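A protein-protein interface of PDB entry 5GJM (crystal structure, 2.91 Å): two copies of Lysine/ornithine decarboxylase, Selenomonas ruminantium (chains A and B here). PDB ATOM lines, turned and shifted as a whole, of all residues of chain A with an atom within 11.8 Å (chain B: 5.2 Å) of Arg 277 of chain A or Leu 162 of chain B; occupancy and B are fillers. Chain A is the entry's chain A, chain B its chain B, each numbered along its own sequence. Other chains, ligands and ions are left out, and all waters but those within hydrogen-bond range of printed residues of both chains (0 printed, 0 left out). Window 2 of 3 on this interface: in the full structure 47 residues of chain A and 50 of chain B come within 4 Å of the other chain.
The side-chain amino group (NZ) of Lys 275 of chain A lies within salt-bridge range of the side-chain carboxylate (OD1) of Asp 116 of chain B (3.3 Å).
O of Asp 116 of chain B sits at hydrogen-bond distance from NH1 of Arg 277 of chain A (3.0 Å).
The backbone carbonyl oxygen (O) of Thr 274 of chain A lies close to the side-chain carboxylate (OD1) of Asp 117 of chain B (2.9 Å).
N of Lys 275 of chain A sits at hydrogen-bond distance from O of Trp 282 of chain A, at 2.9 Å.
N of Gly 153 of chain B sits at hydrogen-bond distance from OD2 of Asp 116 of chain B (3.5 Å).
Among the printed residues, merely in contact across the chains: Lys 275 of chain A with Asp 117 of chain B (3.5 Å), Arg 277 of chain A with Gly 153 of chain B (3.9 Å), Arg 277 of chain A with Ala 154 of chain B (3.7 Å), Arg 277 of chain A with Pro 155 of chain B (3.3 Å) and Arg 277 of chain A with Leu 162 of chain B (3.8 Å).
Printed residues of chain B within 4 Å of Thr 274 of chain A: Asp 117.
Of the printed residues of chain B, Lys 275 of chain A touches Asp 116 (3.3 Å) and Asp 117 (3.5 Å).
Of chain B, only Asp 116, Gly 153, Ala 154, Pro 155 and Leu 162 come within 4 Å of Arg 277 of chain A.
Pro 281 of chain A touches none of the printed residues of chain B.
Printed residues of chain A within 4 Å of Asp 116 of chain B: Lys 275 and Arg 277.
Of chain A, only Thr 274 and Lys 275 come within 4 Å of Asp 117 of chain B.
Pro 118 of chain B touches none of the printed residues of chain A.
Gly 153 of chain B touches just one residue of chain A: Arg 277.
Ala 154 of chain B touches one residue of chain A.
Pro 155 of chain B touches just one residue of chain A: Arg 277 (3.3 Å).
No residue of chain A comes within 4 Å of Ala 159 of chain B.
Leu 160 of chain B touches none of the printed residues of chain A.
Leu 162 of chain B touches just one residue of chain A: Arg 277.
No residue of chain A comes within 4 Å of Leu 163 of chain B.
No residue of chain A comes within 4 Å of Ala 165 of chain B.
No residue of chain A comes within 4 Å of Ala 166 of chain B.
The nearest residue of chain B that does not touch Arg 277 of chain A is Glu 158 of chain B (4.1 Å).
The nearest residue of chain A that does not touch Leu 162 of chain B is Thr 276 of chain A (9.3 Å).
Of the 16 printed residues of chain A, 3 touch a printed residue of chain B.
Along chain A the printed residues that touch a printed residue of chain B span positions 274 to 277.
No position is printed for both chains.
Of the 8 pairs that touch across the chains among the printed residues, none has its exchanged pair printed and touching as well.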
ATOM      1  N   GLY A 273      22.663   1.352  12.731  1.00  0.00           N
ATOM      2  CA  GLY A 273      21.724   2.384  12.309  1.00  0.00           C
ATOM      3  C   GLY A 273      20.643   1.799  11.426  1.00  0.00           C
ATOM      4  O   GLY A 273      20.738   0.645  10.997  1.00  0.00           O
ATOM      5  N   THR A 274      19.602   2.601  11.198  1.00  0.00           N
ATOM      6  CA  THR A 274      18.463   2.245  10.359  1.00  0.00           C
ATOM      7  C   THR A 274      18.107   3.453   9.544  1.00  0.00           C
ATOM      8  O   THR A 274      18.128   4.555  10.067  1.00  0.00           O
ATOM      9  CB  THR A 274      17.237   1.852  11.197  1.00  0.00           C
ATOM     10  OG1 THR A 274      17.573   0.707  11.985  1.00  0.00           O
ATOM     11  CG2 THR A 274      16.030   1.514  10.298  1.00  0.00           C
ATOM     12  N   LYS A 275      17.816   3.251   8.264  1.00  0.00           N
ATOM     13  CA  LYS A 275      17.156   4.273   7.463  1.00  0.00           C
ATOM     14  C   LYS A 275      15.797   3.751   7.021  1.00  0.00           C
ATOM     15  O   LYS A 275      15.658   2.615   6.569  1.00  0.00           O
ATOM     16  CB  LYS A 275      18.006   4.683   6.278  1.00  0.00           C
ATOM     17  CG  LYS A 275      19.451   4.954   6.644  1.00  0.00           C
ATOM     18  CD  LYS A 275      20.125   5.695   5.510  1.00  0.00           C
ATOM     19  CE  LYS A 275      21.601   5.922   5.777  1.00  0.00           C
ATOM     20  NZ  LYS A 275      21.876   7.135   6.620  1.00  0.00           N
ATOM     21  N   THR A 276      14.786   4.590   7.201  1.00  0.00           N
ATOM     22  CA  THR A 276      13.406   4.214   6.935  1.00  0.00           C
ATOM     23  C   THR A 276      12.719   5.144   5.909  1.00  0.00           C
ATOM     24  O   THR A 276      11.518   5.015   5.691  1.00  0.00           O
ATOM     25  CB  THR A 276      12.629   4.139   8.273  1.00  0.00           C
ATOM     26  OG1 THR A 276      11.511   3.252   8.133  1.00  0.00           O
ATOM     27  CG2 THR A 276      12.183   5.549   8.768  1.00  0.00           C
ATOM     28  N   ARG A 277      13.479   6.036   5.261  1.00  0.00           N
ATOM     29  CA  ARG A 277      12.915   6.955   4.275  1.00  0.00           C
ATOM     30  C   ARG A 277      12.662   6.316   2.925  1.00  0.00           C
ATOM     31  O   ARG A 277      11.662   6.649   2.282  1.00  0.00           O
ATOM     32  CB  ARG A 277      13.782   8.201   4.091  1.00  0.00           C
ATOM     33  CG  ARG A 277      13.401   9.275   5.076  1.00  0.00           C
ATOM     34  CD  ARG A 277      13.871  10.652   4.666  1.00  0.00           C
ATOM     35  NE  ARG A 277      14.167  11.405   5.886  1.00  0.00           N
ATOM     36  CZ  ARG A 277      15.344  11.423   6.520  1.00  0.00           C
ATOM     37  NH1 ARG A 277      15.460  12.128   7.641  1.00  0.00           N
ATOM     38  NH2 ARG A 277      16.412  10.761   6.052  1.00  0.00           N
ATOM     39  N   GLY A 278      13.557   5.420   2.491  1.00  0.00           N
ATOM     40  CA  GLY A 278      13.351   4.631   1.255  1.00  0.00           C
ATOM     41  C   GLY A 278      12.141   3.696   1.323  1.00  0.00           C
ATOM     42  O   GLY A 278      11.457   3.614   2.345  1.00  0.00           O
ATOM     43  N   GLU A 279      11.865   2.987   0.235  1.00  0.00           N
ATOM     44  CA  GLU A 279      10.753   2.033   0.230  1.00  0.00           C
ATOM     45  C   GLU A 279      11.217   0.697   0.867  1.00  0.00           C
ATOM     46  O   GLU A 279      10.456   0.026   1.577  1.00  0.00           O
ATOM     47  CB  GLU A 279      10.202   1.871  -1.196  1.00  0.00           C
ATOM     48  CG  GLU A 279       8.677   1.812  -1.275  1.00  0.00           C
ATOM     49  CD  GLU A 279       8.118   0.465  -0.834  1.00  0.00           C
ATOM     50  OE1 GLU A 279       7.568   0.366   0.288  1.00  0.00           O
ATOM     51  OE2 GLU A 279       8.240  -0.511  -1.608  1.00  0.00           O
ATOM     52  N   GLN A 280      12.475   0.339   0.599  1.00  0.00           N
ATOM     53  CA  GLN A 280      13.171  -0.764   1.263  1.00  0.00           C
ATOM     54  C   GLN A 280      13.737  -0.293   2.583  1.00  0.00           C
ATOM     55  O   GLN A 280      14.344   0.772   2.615  1.00  0.00           O
ATOM     56  CB  GLN A 280      14.400  -1.206   0.454  1.00  0.00           C
ATOM     57  CG  GLN A 280      14.179  -2.170  -0.694  1.00  0.00           C
ATOM     58  CD  GLN A 280      15.446  -2.939  -1.034  1.00  0.00           C
ATOM     59  OE1 GLN A 280      16.463  -2.834  -0.352  1.00  0.00           O
ATOM     60  NE2 GLN A 280      15.389  -3.721  -2.087  1.00  0.00           N
ATOM     61  N   PRO A 281      13.641  -1.108   3.653  1.00  0.00           N
ATOM     62  CA  PRO A 281      14.340  -0.718   4.877  1.00  0.00           C
ATOM     63  C   PRO A 281      15.840  -0.887   4.689  1.00  0.00           C
ATOM     64  O   PRO A 281      16.264  -1.765   3.928  1.00  0.00           O
ATOM     65  CB  PRO A 281      13.821  -1.703   5.932  1.00  0.00           C
ATOM     66  CG  PRO A 281      13.029  -2.728   5.190  1.00  0.00           C
ATOM     67  CD  PRO A 281      13.204  -2.507   3.725  1.00  0.00           C
ATOM     68  N   TRP A 282      16.612  -0.063   5.393  1.00  0.00           N
ATOM     69  CA  TRP A 282      18.068   0.037   5.234  1.00  0.00           C
ATOM     70  C   TRP A 282      18.708  -0.246   6.588  1.00  0.00           C
ATOM     71  O   TRP A 282      18.379   0.449   7.566  1.00  0.00           O
ATOM     72  CB  TRP A 282      18.437   1.455   4.787  1.00  0.00           C
ATOM     73  CG  TRP A 282      18.995   1.621   3.393  1.00  0.00           C
ATOM     74  CD1 TRP A 282      18.291   1.675   2.208  1.00  0.00           C
ATOM     75  CD2 TRP A 282      20.374   1.821   3.045  1.00  0.00           C
ATOM     76  NE1 TRP A 282      19.162   1.875   1.143  1.00  0.00           N
ATOM     77  CE2 TRP A 282      20.437   1.976   1.630  1.00  0.00           C
ATOM     78  CE3 TRP A 282      21.554   1.870   3.785  1.00  0.00           C
ATOM     79  CZ2 TRP A 282      21.623   2.172   0.957  1.00  0.00           C
ATOM     80  CZ3 TRP A 282      22.731   2.072   3.124  1.00  0.00           C
ATOM     81  CH2 TRP A 282      22.764   2.221   1.713  1.00  0.00           C
ATOM     82  N   TYR A 283      19.587  -1.258   6.652  1.00  0.00           N
ATOM     83  CA  TYR A 283      20.293  -1.613   7.894  1.00  0.00           C
ATOM     84  C   TYR A 283      21.784  -1.351   7.734  1.00  0.00           C
ATOM     85  O   TYR A 283      22.380  -1.808   6.780  1.00  0.00           O
ATOM     86  CB  TYR A 283      20.053  -3.077   8.256  1.00  0.00           C
ATOM     87  CG  TYR A 283      18.598  -3.378   8.481  1.00  0.00           C
ATOM     88  CD1 TYR A 283      17.925  -2.856   9.573  1.00  0.00           C
ATOM     89  CD2 TYR A 283      17.880  -4.153   7.580  1.00  0.00           C
ATOM     90  CE1 TYR A 283      16.584  -3.101   9.766  1.00  0.00           C
ATOM     91  CE2 TYR A 283      16.542  -4.409   7.774  1.00  0.00           C
ATOM     92  CZ  TYR A 283      15.897  -3.880   8.869  1.00  0.00           C
ATOM     93  OH  TYR A 283      14.556  -4.126   9.087  1.00  0.00           O
ATOM     94  N   ILE A 284      22.385  -0.598   8.648  1.00  0.00           N
ATOM     95  CA  ILE A 284      23.827  -0.363   8.600  1.00  0.00           C
ATOM     96  C   ILE A 284      24.436  -1.282   9.629  1.00  0.00           C
ATOM     97  O   ILE A 284      23.990  -1.296  10.770  1.00  0.00           O
ATOM     98  CB  ILE A 284      24.234   1.095   8.914  1.00  0.00           C
ATOM     99  CG1 ILE A 284      23.597   2.095   7.922  1.00  0.00           C
ATOM    100  CG2 ILE A 284      25.750   1.224   8.916  1.00  0.00           C
ATOM    101  CD1 ILE A 284      24.213   2.122   6.525  1.00  0.00           C
ATOM    102  N   LYS A 314      10.767  -8.421   4.292  1.00  0.00           N
ATOM    103  CA  LYS A 314      10.601  -7.413   3.291  1.00  0.00           C
ATOM    104  C   LYS A 314      11.931  -7.385   2.644  1.00  0.00           C
ATOM    105  O   LYS A 314      12.910  -7.577   3.325  1.00  0.00           O
ATOM    106  CB  LYS A 314      10.353  -6.081   3.967  1.00  0.00           C
ATOM    107  CG  LYS A 314       9.175  -5.314   3.430  1.00  0.00           C
ATOM    108  CD  LYS A 314       9.416  -3.830   3.526  1.00  0.00           C
ATOM    109  CE  LYS A 314       8.423  -3.167   4.459  1.00  0.00           C
ATOM    110  NZ  LYS A 314       9.069  -2.142   5.325  1.00  0.00           N
ATOM    111  N   PRO A 315      12.003  -7.084   1.368  1.00  0.00           N
ATOM    112  CA  PRO A 315      13.311  -6.872   0.778  1.00  0.00           C
ATOM    113  C   PRO A 315      13.966  -5.692   1.453  1.00  0.00           C
ATOM    114  O   PRO A 315      13.417  -4.621   1.587  1.00  0.00           O
ATOM    115  CB  PRO A 315      12.979  -6.538  -0.656  1.00  0.00           C
ATOM    116  CG  PRO A 315      11.736  -7.295  -0.924  1.00  0.00           C
ATOM    117  CD  PRO A 315      11.024  -7.517   0.370  1.00  0.00           C
ATOM    118  N   SER A 316      15.191  -5.910   1.864  1.00  0.00           N
ATOM    119  CA  SER A 316      15.908  -4.942   2.681  1.00  0.00           C
ATOM    120  C   SER A 316      17.329  -4.828   2.199  1.00  0.00           C
ATOM    121  O   SER A 316      17.871  -5.744   1.584  1.00  0.00           O
ATOM    122  CB  SER A 316      15.888  -5.365   4.156  1.00  0.00           C
ATOM    123  OG  SER A 316      14.640  -5.964   4.516  1.00  0.00           O
ATOM    124  N   THR A 317      17.916  -3.676   2.494  1.00  0.00           N
ATOM    125  CA  THR A 317      19.275  -3.336   2.086  1.00  0.00           C
ATOM    126  C   THR A 317      20.174  -3.291   3.329  1.00  0.00           C
ATOM    127  O   THR A 317      19.748  -2.831   4.387  1.00  0.00           O
ATOM    128  CB  THR A 317      19.276  -2.011   1.276  1.00  0.00           C
ATOM    129  OG1 THR A 317      18.876  -2.288  -0.073  1.00  0.00           O
ATOM    130  CG2 THR A 317      20.644  -1.343   1.229  1.00  0.00           C
ATOM    131  N   PHE B 115      24.123  14.275  12.138  1.00  0.00           N
ATOM    132  CA  PHE B 115      23.115  13.201  11.960  1.00  0.00           C
ATOM    133  C   PHE B 115      22.091  13.526  10.855  1.00  0.00           C
ATOM    134  O   PHE B 115      21.844  14.693  10.536  1.00  0.00           O
ATOM    135  CB  PHE B 115      22.401  12.890  13.289  1.00  0.00           C
ATOM    136  CG  PHE B 115      21.386  13.922  13.706  1.00  0.00           C
ATOM    137  CD1 PHE B 115      21.774  15.211  14.039  1.00  0.00           C
ATOM    138  CD2 PHE B 115      20.037  13.598  13.793  1.00  0.00           C
ATOM    139  CE1 PHE B 115      20.835  16.161  14.441  1.00  0.00           C
ATOM    140  CE2 PHE B 115      19.092  14.549  14.184  1.00  0.00           C
ATOM    141  CZ  PHE B 115      19.490  15.831  14.517  1.00  0.00           C
ATOM    142  N   ASP B 116      21.526  12.485  10.254  1.00  0.00           N
ATOM    143  CA  ASP B 116      20.466  12.662   9.251  1.00  0.00           C
ATOM    144  C   ASP B 116      19.182  11.883   9.512  1.00  0.00           C
ATOM    145  O   ASP B 116      18.239  12.029   8.756  1.00  0.00           O
ATOM    146  CB  ASP B 116      20.988  12.417   7.798  1.00  0.00           C
ATOM    147  CG  ASP B 116      21.543  10.980   7.541  1.00  0.00           C
ATOM    148  OD1 ASP B 116      20.971   9.955   7.995  1.00  0.00           O
ATOM    149  OD2 ASP B 116      22.564  10.889   6.803  1.00  0.00           O
ATOM    150  N   ASP B 117      19.129  11.095  10.581  1.00  0.00           N
ATOM    151  CA  ASP B 117      18.094  10.085  10.753  1.00  0.00           C
ATOM    152  C   ASP B 117      17.682  10.150  12.187  1.00  0.00           C
ATOM    153  O   ASP B 117      18.549  10.371  13.030  1.00  0.00           O
ATOM    154  CB  ASP B 117      18.648   8.689  10.417  1.00  0.00           C
ATOM    155  CG  ASP B 117      17.541   7.645  10.155  1.00  0.00           C
ATOM    156  OD1 ASP B 117      17.045   7.046  11.155  1.00  0.00           O
ATOM    157  OD2 ASP B 117      17.173   7.409   8.960  1.00  0.00           O
ATOM    158  N   PRO B 118      16.368   9.974  12.479  1.00  0.00           N
ATOM    159  CA  PRO B 118      15.890  10.021  13.867  1.00  0.00           C
ATOM    160  C   PRO B 118      16.224   8.799  14.729  1.00  0.00           C
ATOM    161  O   PRO B 118      16.103   8.900  15.950  1.00  0.00           O
ATOM    162  CB  PRO B 118      14.373  10.162  13.696  1.00  0.00           C
ATOM    163  CG  PRO B 118      14.108   9.394  12.468  1.00  0.00           C
ATOM    164  CD  PRO B 118      15.225   9.823  11.556  1.00  0.00           C
ATOM    165  N   ILE B 121      19.219   9.839  16.895  1.00  0.00           N
ATOM    166  CA  ILE B 121      18.944  10.742  18.052  1.00  0.00           C
ATOM    167  C   ILE B 121      18.814   9.956  19.352  1.00  0.00           C
ATOM    168  O   ILE B 121      19.420  10.296  20.368  1.00  0.00           O
ATOM    169  CB  ILE B 121      17.627  11.559  17.864  1.00  0.00           C
ATOM    170  CG1 ILE B 121      17.785  12.559  16.716  1.00  0.00           C
ATOM    171  CG2 ILE B 121      17.241  12.317  19.132  1.00  0.00           C
ATOM    172  CD1 ILE B 121      16.491  13.161  16.236  1.00  0.00           C
ATOM    173  N   VAL B 135      22.382  18.977  11.663  1.00  0.00           N
ATOM    174  CA  VAL B 135      21.674  18.094  10.730  1.00  0.00           C
ATOM    175  C   VAL B 135      22.340  18.191   9.371  1.00  0.00           C
ATOM    176  O   VAL B 135      22.609  19.295   8.881  1.00  0.00           O
ATOM    177  CB  VAL B 135      20.161  18.431  10.615  1.00  0.00           C
ATOM    178  CG1 VAL B 135      19.444  17.534   9.625  1.00  0.00           C
ATOM    179  CG2 VAL B 135      19.504  18.177  11.928  1.00  0.00           C
ATOM    180  N   GLY B 153      21.889  12.375   3.715  1.00  0.00           N
ATOM    181  CA  GLY B 153      21.347  13.692   3.878  1.00  0.00           C
ATOM    182  C   GLY B 153      19.892  13.533   4.207  1.00  0.00           C
ATOM    183  O   GLY B 153      19.343  12.465   4.063  1.00  0.00           O
ATOM    184  N   ALA B 154      19.241  14.587   4.638  1.00  0.00           N
ATOM    185  CA  ALA B 154      17.881  14.506   5.063  1.00  0.00           C
ATOM    186  C   ALA B 154      17.100  15.565   4.383  1.00  0.00           C
ATOM    187  O   ALA B 154      17.588  16.626   4.131  1.00  0.00           O
ATOM    188  CB  ALA B 154      17.836  14.728   6.522  1.00  0.00           C
ATOM    189  N   PRO B 155      15.860  15.284   4.067  1.00  0.00           N
ATOM    190  CA  PRO B 155      15.069  16.213   3.269  1.00  0.00           C
ATOM    191  C   PRO B 155      14.908  17.555   3.945  1.00  0.00           C
ATOM    192  O   PRO B 155      14.633  17.641   5.118  1.00  0.00           O
ATOM    193  CB  PRO B 155      13.736  15.509   3.181  1.00  0.00           C
ATOM    194  CG  PRO B 155      14.110  14.088   3.179  1.00  0.00           C
ATOM    195  CD  PRO B 155      15.207  13.977   4.165  1.00  0.00           C
ATOM    196  N   GLU B 158      12.235  18.092   6.257  1.00  0.00           N
ATOM    197  CA  GLU B 158      12.283  17.451   7.556  1.00  0.00           C
ATOM    198  C   GLU B 158      13.405  17.930   8.485  1.00  0.00           C
ATOM    199  O   GLU B 158      13.503  17.477   9.596  1.00  0.00           O
ATOM    200  CB  GLU B 158      12.289  15.935   7.418  1.00  0.00           C
ATOM    201  CG  GLU B 158      12.218  15.249   8.764  1.00  0.00           C
ATOM    202  CD  GLU B 158      11.261  14.085   8.800  1.00  0.00           C
ATOM    203  OE1 GLU B 158      10.045  14.304   8.618  1.00  0.00           O
ATOM    204  OE2 GLU B 158      11.734  12.954   9.040  1.00  0.00           O
ATOM    205  N   ALA B 159      14.231  18.856   8.028  1.00  0.00           N
ATOM    206  CA  ALA B 159      15.402  19.317   8.766  1.00  0.00           C
ATOM    207  C   ALA B 159      15.074  19.890  10.132  1.00  0.00           C
ATOM    208  O   ALA B 159      15.763  19.607  11.110  1.00  0.00           O
ATOM    209  CB  ALA B 159      16.136  20.368   7.964  1.00  0.00           C
ATOM    210  N   LEU B 160      14.029  20.706  10.213  1.00  0.00           N
ATOM    211  CA  LEU B 160      13.727  21.393  11.472  1.00  0.00           C
ATOM    212  C   LEU B 160      13.054  20.503  12.511  1.00  0.00           C
ATOM    213  O   LEU B 160      13.328  20.631  13.703  1.00  0.00           O
ATOM    214  CB  LEU B 160      12.898  22.644  11.221  1.00  0.00           C
ATOM    215  CG  LEU B 160      13.583  23.691  10.356  1.00  0.00           C
ATOM    216  CD1 LEU B 160      12.752  24.956  10.392  1.00  0.00           C
ATOM    217  CD2 LEU B 160      15.021  23.990  10.768  1.00  0.00           C
ATOM    218  N   ASP B 161      12.176  19.617  12.049  1.00  0.00           N
ATOM    219  CA  ASP B 161      11.543  18.592  12.897  1.00  0.00           C
ATOM    220  C   ASP B 161      12.545  17.663  13.579  1.00  0.00           C
ATOM    221  O   ASP B 161      12.356  17.263  14.735  1.00  0.00           O
ATOM    222  CB  ASP B 161      10.606  17.750  12.038  1.00  0.00           C
ATOM    223  CG  ASP B 161       9.355  18.527  11.572  1.00  0.00           C
ATOM    224  OD1 ASP B 161       9.117  19.679  12.036  1.00  0.00           O
ATOM    225  OD2 ASP B 161       8.603  17.956  10.742  1.00  0.00           O
ATOM    226  N   LEU B 162      13.592  17.339  12.832  1.00  0.00           N
ATOM    227  CA  LEU B 162      14.755  16.546  13.233  1.00  0.00           C
ATOM    228  C   LEU B 162      15.610  17.162  14.323  1.00  0.00           C
ATOM    229  O   LEU B 162      16.042  16.479  15.213  1.00  0.00           O
ATOM    230  CB  LEU B 162      15.619  16.308  11.999  1.00  0.00           C
ATOM    231  CG  LEU B 162      16.008  14.931  11.464  1.00  0.00           C
ATOM    232  CD1 LEU B 162      15.000  13.863  11.808  1.00  0.00           C
ATOM    233  CD2 LEU B 162      16.202  15.031   9.974  1.00  0.00           C
ATOM    234  N   LEU B 163      15.849  18.460  14.247  1.00  0.00           N
ATOM    235  CA  LEU B 163      16.541  19.229  15.308  1.00  0.00           C
ATOM    236  C   LEU B 163      15.694  19.399  16.569  1.00  0.00           C
ATOM    237  O   LEU B 163      16.205  19.330  17.663  1.00  0.00           O
ATOM    238  CB  LEU B 163      16.973  20.610  14.793  1.00  0.00           C
ATOM    239  CG  LEU B 163      18.206  20.611  13.877  1.00  0.00           C
ATOM    240  CD1 LEU B 163      18.391  21.912  13.094  1.00  0.00           C
ATOM    241  CD2 LEU B 163      19.468  20.274  14.660  1.00  0.00           C
ATOM    242  N   LYS B 164      14.398  19.624  16.410  1.00  0.00           N
ATOM    243  CA  LYS B 164      13.478  19.705  17.545  1.00  0.00           C
ATOM    244  C   LYS B 164      13.314  18.377  18.298  1.00  0.00           C
ATOM    245  O   LYS B 164      13.221  18.371  19.526  1.00  0.00           O
ATOM    246  CB  LYS B 164      12.121  20.188  17.065  1.00  0.00           C
ATOM    247  CG  LYS B 164      11.188  20.613  18.178  1.00  0.00           C
ATOM    248  CD  LYS B 164      10.234  21.665  17.634  1.00  0.00           C
ATOM    249  CE  LYS B 164       8.785  21.489  18.109  1.00  0.00           C
ATOM    250  NZ  LYS B 164       7.827  22.080  17.117  1.00  0.00           N
ATOM    251  N   ALA B 165      13.264  17.269  17.557  1.00  0.00           N
ATOM    252  CA  ALA B 165      13.345  15.928  18.155  1.00  0.00           C
ATOM    253  C   ALA B 165      14.627  15.738  18.948  1.00  0.00           C
ATOM    254  O   ALA B 165      14.614  15.154  20.031  1.00  0.00           O
ATOM    255  CB  ALA B 165      13.265  14.869  17.082  1.00  0.00           C
ATOM    256  N   ALA B 166      15.734  16.226  18.380  1.00  0.00           N
ATOM    257  CA  ALA B 166      17.047  16.221  19.042  1.00  0.00           C
ATOM    258  C   ALA B 166      17.039  17.100  20.305  1.00  0.00           C
ATOM    259  O   ALA B 166      17.374  16.646  21.402  1.00  0.00           O
ATOM    260  CB  ALA B 166      18.130  16.671  18.066  1.00  0.00           C
